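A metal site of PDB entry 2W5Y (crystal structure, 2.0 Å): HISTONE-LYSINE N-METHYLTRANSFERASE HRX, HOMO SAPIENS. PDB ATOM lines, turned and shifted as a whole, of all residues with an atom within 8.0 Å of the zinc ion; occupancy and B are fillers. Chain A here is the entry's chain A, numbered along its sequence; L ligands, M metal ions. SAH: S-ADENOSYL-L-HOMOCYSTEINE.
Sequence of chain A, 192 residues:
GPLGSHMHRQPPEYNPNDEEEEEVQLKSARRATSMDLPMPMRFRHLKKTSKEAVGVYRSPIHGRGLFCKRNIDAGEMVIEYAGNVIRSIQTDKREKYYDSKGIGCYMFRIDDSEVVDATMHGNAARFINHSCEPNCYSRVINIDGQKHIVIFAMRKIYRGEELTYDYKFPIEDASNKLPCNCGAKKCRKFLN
A nitrogen (N7) of the ligand sits at hydrogen-bond distance from the backbone NH of His 130 (2.9 Å).
The side-chain sulfur (SG) of Cys 180 lies close to a nitrogen (N6) of the ligand, at 3.7 Å.
N6 of the ligand is in hydrogen-bond range of O of His 130.
N of Asn 181 sits at hydrogen-bond distance from N1 of the ligand, at 2.8 Å.
OG of Ser 131 lies close to SG of Cys 182 (3.7 Å).
O of Lys 189 lies within hydrogen-bond range of N of Cys 180, at 2.9 Å.
NH1 of Arg 188 sits close to O of Cys 132.
The side-chain sulfur (SG) of Cys 182 sits close to the backbone NH (N) of Ala 184, 3.6 Å away.
The side-chain sulfur (SG) of Cys 187 lies close to the backbone NH (N) of Lys 189 (3.1 Å).
The side-chain sulfur (SG) of Cys 132 lies close to a ring nitrogen (NE2) of His 130 (3.5 Å).
Merely in contact with the zinc ion: Arg 188 (3.9 Å).
Within 4 Å of the zinc ion: Cys 132, Cys 180, Cys 182, Cys 187 and Arg 188.
The nearest printed residue that does not touch the zinc ion is His 130 (4.4 Å).
The side-chain sulfur (SG) of Cys 180 binds the zinc ion, at 2.3 Å.
The zinc ion is bound by SG of Cys 182.
SG of Cys 132 binds the zinc ion, 2.5 Å away.
The side-chain sulfur (SG) of Cys 187 is bound to the zinc ion, at 2.7 Å.
The zinc ion has four donor atoms within binding distance.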
ATOM      1  N   ILE A  61      10.949 -10.524 -21.795  1.00  0.00           N
ATOM      2  CA  ILE A  61      12.409 -10.559 -21.817  1.00  0.00           C
ATOM      3  C   ILE A  61      12.851 -11.143 -23.156  1.00  0.00           C
ATOM      4  O   ILE A  61      13.576 -10.509 -23.917  1.00  0.00           O
ATOM      5  CB  ILE A  61      12.988 -11.393 -20.645  1.00  0.00           C
ATOM      6  CG1 ILE A  61      12.666 -10.704 -19.308  1.00  0.00           C
ATOM      7  CG2 ILE A  61      14.495 -11.599 -20.800  1.00  0.00           C
ATOM      8  CD1 ILE A  61      12.906 -11.601 -18.085  1.00  0.00           C
ATOM      9  N   HIS A 130      17.339 -15.439 -18.792  1.00  0.00           N
ATOM     10  CA  HIS A 130      18.376 -14.849 -17.966  1.00  0.00           C
ATOM     11  C   HIS A 130      17.907 -13.527 -17.392  1.00  0.00           C
ATOM     12  O   HIS A 130      17.136 -12.807 -18.006  1.00  0.00           O
ATOM     13  CB  HIS A 130      19.660 -14.619 -18.777  1.00  0.00           C
ATOM     14  CG  HIS A 130      20.605 -13.653 -18.116  1.00  0.00           C
ATOM     15  ND1 HIS A 130      21.600 -14.063 -17.263  1.00  0.00           N
ATOM     16  CD2 HIS A 130      20.656 -12.303 -18.136  1.00  0.00           C
ATOM     17  CE1 HIS A 130      22.249 -13.008 -16.803  1.00  0.00           C
ATOM     18  NE2 HIS A 130      21.687 -11.921 -17.325  1.00  0.00           N
ATOM     19  N   SER A 131      18.387 -13.211 -16.196  1.00  0.00           N
ATOM     20  CA  SER A 131      18.210 -11.879 -15.639  1.00  0.00           C
ATOM     21  C   SER A 131      19.383 -11.528 -14.736  1.00  0.00           C
ATOM     22  O   SER A 131      19.883 -12.364 -13.978  1.00  0.00           O
ATOM     23  CB  SER A 131      16.922 -11.755 -14.849  1.00  0.00           C
ATOM     24  OG  SER A 131      16.882 -10.504 -14.191  1.00  0.00           O
ATOM     25  N   CYS A 132      19.821 -10.273 -14.820  1.00  0.00           N
ATOM     26  CA  CYS A 132      20.877  -9.786 -13.954  1.00  0.00           C
ATOM     27  C   CYS A 132      20.368  -9.619 -12.517  1.00  0.00           C
ATOM     28  O   CYS A 132      21.169  -9.569 -11.579  1.00  0.00           O
ATOM     29  CB  CYS A 132      21.456  -8.484 -14.510  1.00  0.00           C
ATOM     30  SG  CYS A 132      22.119  -8.659 -16.197  1.00  0.00           S
ATOM     31  N   GLU A 133      19.046  -9.541 -12.339  1.00  0.00           N
ATOM     32  CA  GLU A 133      18.408  -9.513 -11.013  1.00  0.00           C
ATOM     33  C   GLU A 133      17.478 -10.723 -10.822  1.00  0.00           C
ATOM     34  O   GLU A 133      16.251 -10.577 -10.798  1.00  0.00           O
ATOM     35  CB  GLU A 133      17.605  -8.225 -10.809  1.00  0.00           C
ATOM     36  CG  GLU A 133      18.352  -6.963 -11.186  1.00  0.00           C
ATOM     37  CD  GLU A 133      18.729  -6.096  -9.996  1.00  0.00           C
ATOM     38  OE1 GLU A 133      19.744  -6.411  -9.329  1.00  0.00           O
ATOM     39  OE2 GLU A 133      18.038  -5.080  -9.758  1.00  0.00           O
ATOM     40  N   PRO A 179      23.318  -8.700 -26.412  1.00  0.00           N
ATOM     41  CA  PRO A 179      22.554  -7.839 -25.522  1.00  0.00           C
ATOM     42  C   PRO A 179      21.615  -8.517 -24.537  1.00  0.00           C
ATOM     43  O   PRO A 179      21.017  -9.526 -24.855  1.00  0.00           O
ATOM     44  CB  PRO A 179      21.813  -6.951 -26.491  1.00  0.00           C
ATOM     45  CG  PRO A 179      21.721  -7.754 -27.766  1.00  0.00           C
ATOM     46  CD  PRO A 179      22.603  -8.929 -27.663  1.00  0.00           C
ATOM     47  N   CYS A 180      21.519  -7.930 -23.355  1.00  0.00           N
ATOM     48  CA  CYS A 180      20.586  -8.363 -22.310  1.00  0.00           C
ATOM     49  C   CYS A 180      19.268  -7.605 -22.233  1.00  0.00           C
ATOM     50  O   CYS A 180      19.242  -6.385 -22.069  1.00  0.00           O
ATOM     51  CB  CYS A 180      21.252  -8.369 -20.930  1.00  0.00           C
ATOM     52  SG  CYS A 180      20.168  -9.008 -19.615  1.00  0.00           S
ATOM     53  N   ASN A 181      18.165  -8.353 -22.295  1.00  0.00           N
ATOM     54  CA  ASN A 181      16.821  -7.766 -22.306  1.00  0.00           C
ATOM     55  C   ASN A 181      16.077  -7.797 -20.950  1.00  0.00           C
ATOM     56  O   ASN A 181      14.881  -7.490 -20.900  1.00  0.00           O
ATOM     57  CB  ASN A 181      15.956  -8.439 -23.386  1.00  0.00           C
ATOM     58  CG  ASN A 181      16.581  -8.372 -24.783  1.00  0.00           C
ATOM     59  OD1 ASN A 181      17.439  -7.528 -25.062  1.00  0.00           O
ATOM     60  ND2 ASN A 181      16.142  -9.263 -25.673  1.00  0.00           N
ATOM     61  N   CYS A 182      16.760  -8.154 -19.870  1.00  0.00           N
ATOM     62  CA  CYS A 182      16.079  -8.301 -18.574  1.00  0.00           C
ATOM     63  C   CYS A 182      15.609  -6.959 -18.022  1.00  0.00           C
ATOM     64  O   CYS A 182      16.068  -5.892 -18.447  1.00  0.00           O
ATOM     65  CB  CYS A 182      16.964  -9.030 -17.553  1.00  0.00           C
ATOM     66  SG  CYS A 182      18.087  -7.984 -16.588  1.00  0.00           S
ATOM     67  N   GLY A 183      14.681  -6.996 -17.069  1.00  0.00           N
ATOM     68  CA  GLY A 183      14.110  -5.764 -16.539  1.00  0.00           C
ATOM     69  C   GLY A 183      15.058  -4.975 -15.651  1.00  0.00           C
ATOM     70  O   GLY A 183      15.025  -3.740 -15.642  1.00  0.00           O
ATOM     71  N   ALA A 184      15.899  -5.719 -14.921  1.00  0.00           N
ATOM     72  CA  ALA A 184      16.861  -5.196 -13.953  1.00  0.00           C
ATOM     73  C   ALA A 184      17.251  -3.728 -14.078  1.00  0.00           C
ATOM     74  O   ALA A 184      17.587  -3.254 -15.169  1.00  0.00           O
ATOM     75  CB  ALA A 184      18.116  -6.050 -13.983  1.00  0.00           C
ATOM     76  N   LYS A 185      17.249  -3.025 -12.952  1.00  0.00           N
ATOM     77  CA  LYS A 185      17.768  -1.672 -12.893  1.00  0.00           C
ATOM     78  C   LYS A 185      19.292  -1.727 -12.876  1.00  0.00           C
ATOM     79  O   LYS A 185      19.958  -0.796 -13.312  1.00  0.00           O
ATOM     80  CB  LYS A 185      17.238  -0.923 -11.665  1.00  0.00           C
ATOM     81  CG  LYS A 185      17.548   0.562 -11.661  1.00  0.00           C
ATOM     82  N   LYS A 186      19.834  -2.832 -12.375  1.00  0.00           N
ATOM     83  CA  LYS A 186      21.273  -3.052 -12.330  1.00  0.00           C
ATOM     84  C   LYS A 186      21.772  -3.881 -13.517  1.00  0.00           C
ATOM     85  O   LYS A 186      22.852  -4.467 -13.466  1.00  0.00           O
ATOM     86  CB  LYS A 186      21.672  -3.737 -11.016  1.00  0.00           C
ATOM     87  CG  LYS A 186      21.570  -2.856  -9.779  1.00  0.00           C
ATOM     88  CD  LYS A 186      22.025  -3.609  -8.540  1.00  0.00           C
ATOM     89  N   CYS A 187      20.966  -3.942 -14.566  1.00  0.00           N
ATOM     90  CA  CYS A 187      21.287  -4.747 -15.741  1.00  0.00           C
ATOM     91  C   CYS A 187      22.758  -4.645 -16.137  1.00  0.00           C
ATOM     92  O   CYS A 187      23.356  -3.560 -16.057  1.00  0.00           O
ATOM     93  CB  CYS A 187      20.392  -4.359 -16.911  1.00  0.00           C
ATOM     94  SG  CYS A 187      20.681  -5.301 -18.427  1.00  0.00           S
ATOM     95  N   ARG A 188      23.341  -5.765 -16.563  1.00  0.00           N
ATOM     96  CA  ARG A 188      24.735  -5.794 -17.014  1.00  0.00           C
ATOM     97  C   ARG A 188      24.852  -5.480 -18.505  1.00  0.00           C
ATOM     98  O   ARG A 188      25.956  -5.444 -19.056  1.00  0.00           O
ATOM     99  CB  ARG A 188      25.373  -7.151 -16.702  1.00  0.00           C
ATOM    100  CG  ARG A 188      26.119  -7.208 -15.386  1.00  0.00           C
ATOM    101  CD  ARG A 188      26.372  -8.645 -14.945  1.00  0.00           C
ATOM    102  NE  ARG A 188      25.279  -9.146 -14.121  1.00  0.00           N
ATOM    103  CZ  ARG A 188      24.902 -10.423 -14.066  1.00  0.00           C
ATOM    104  NH1 ARG A 188      23.895 -10.767 -13.290  1.00  0.00           N
ATOM    105  NH2 ARG A 188      25.514 -11.337 -14.803  1.00  0.00           N
ATOM    106  N   LYS A 189      23.703  -5.278 -19.153  1.00  0.00           N
ATOM    107  CA  LYS A 189      23.638  -4.881 -20.568  1.00  0.00           C
ATOM    108  C   LYS A 189      23.998  -5.989 -21.566  1.00  0.00           C
ATOM    109  O   LYS A 189      23.546  -5.944 -22.714  1.00  0.00           O
ATOM    110  CB  LYS A 189      24.479  -3.625 -20.818  1.00  0.00           C
ATOM    111  CG  LYS A 189      23.960  -2.382 -20.124  1.00  0.00           C
ATOM    112  N   PHE A 190      24.794  -6.969 -21.151  1.00  0.00           N
ATOM    113  CA  PHE A 190      25.139  -8.089 -22.037  1.00  0.00           C
ATOM    114  C   PHE A 190      25.148  -9.428 -21.307  1.00  0.00           C
ATOM    115  O   PHE A 190      25.708  -9.556 -20.223  1.00  0.00           O
ATOM    116  CB  PHE A 190      26.510  -7.858 -22.691  1.00  0.00           C
ATOM    117  CG  PHE A 190      26.637  -6.531 -23.374  1.00  0.00           C
ATOM    118  CD1 PHE A 190      27.340  -5.500 -22.761  1.00  0.00           C
ATOM    119  CD2 PHE A 190      26.052  -6.297 -24.609  1.00  0.00           C
ATOM    120  CE1 PHE A 190      27.460  -4.264 -23.383  1.00  0.00           C
ATOM    121  CE2 PHE A 190      26.173  -5.075 -25.230  1.00  0.00           C
ATOM    122  CZ  PHE A 190      26.877  -4.059 -24.617  1.00  0.00           C
ATOM    123  N   LEU A 191      24.520 -10.436 -21.920  1.00  0.00           N
ATOM    124  CA  LEU A 191      24.510 -11.783 -21.361  1.00  0.00           C
ATOM    125  C   LEU A 191      25.930 -12.284 -21.154  1.00  0.00           C
ATOM    126  O   LEU A 191      26.232 -12.970 -20.174  1.00  0.00           O
ATOM    127  CB  LEU A 191      23.773 -12.750 -22.292  1.00  0.00           C
ATOM    128  CG  LEU A 191      22.293 -12.515 -22.571  1.00  0.00           C
ATOM    129  CD1 LEU A 191      21.743 -13.617 -23.467  1.00  0.00           C
ATOM    130  CD2 LEU A 191      21.529 -12.465 -21.265  1.00  0.00           C
HETATM  131  N   SAH L   1      13.604 -17.378 -24.244  1.00  0.00           N
HETATM  132  CA  SAH L   1      13.981 -18.732 -24.629  1.00  0.00           C
HETATM  133  CB  SAH L   1      14.135 -19.646 -23.399  1.00  0.00           C
HETATM  134  CG  SAH L   1      15.509 -19.580 -22.739  1.00  0.00           C
HETATM  135  SD  SAH L   1      16.772 -20.420 -23.753  1.00  0.00           S
HETATM  136  C   SAH L   1      13.043 -19.292 -25.695  1.00  0.00           C
HETATM  137  O   SAH L   1      12.084 -18.649 -26.118  1.00  0.00           O
HETATM  138  OXT SAH L   1      13.209 -20.402 -26.200  1.00  0.00           O
HETATM  139  C5' SAH L   1      18.043 -19.152 -23.582  1.00  0.00           C
HETATM  140  C4' SAH L   1      18.053 -18.169 -24.763  1.00  0.00           C
HETATM  141  O4' SAH L   1      17.018 -17.201 -24.628  1.00  0.00           O
HETATM  142  C3' SAH L   1      19.362 -17.405 -24.862  1.00  0.00           C
HETATM  143  O3' SAH L   1      20.251 -18.024 -25.751  1.00  0.00           O
HETATM  144  C2' SAH L   1      18.933 -16.070 -25.423  1.00  0.00           C
HETATM  145  O2' SAH L   1      18.868 -16.205 -26.810  1.00  0.00           O
HETATM  146  C1' SAH L   1      17.513 -15.899 -24.916  1.00  0.00           C
HETATM  147  N9  SAH L   1      17.531 -15.091 -23.684  1.00  0.00           N
HETATM  148  C8  SAH L   1      17.371 -15.560 -22.409  1.00  0.00           C
HETATM  149  N7  SAH L   1      17.455 -14.516 -21.548  1.00  0.00           N
HETATM  150  C5  SAH L   1      17.673 -13.387 -22.260  1.00  0.00           C
HETATM  151  C6  SAH L   1      17.840 -12.053 -21.893  1.00  0.00           C
HETATM  152  N6  SAH L   1      17.792 -11.685 -20.617  1.00  0.00           N
HETATM  153  N1  SAH L   1      18.055 -11.097 -22.858  1.00  0.00           N
HETATM  154  C2  SAH L   1      18.096 -11.468 -24.191  1.00  0.00           C
HETATM  155  N3  SAH L   1      17.928 -12.788 -24.558  1.00  0.00           N
HETATM  156  C4  SAH L   1      17.726 -13.736 -23.609  1.00  0.00           C
HETATM  157 ZN    ZN M   1      20.246  -7.811 -17.658  1.00  0.00          ZN
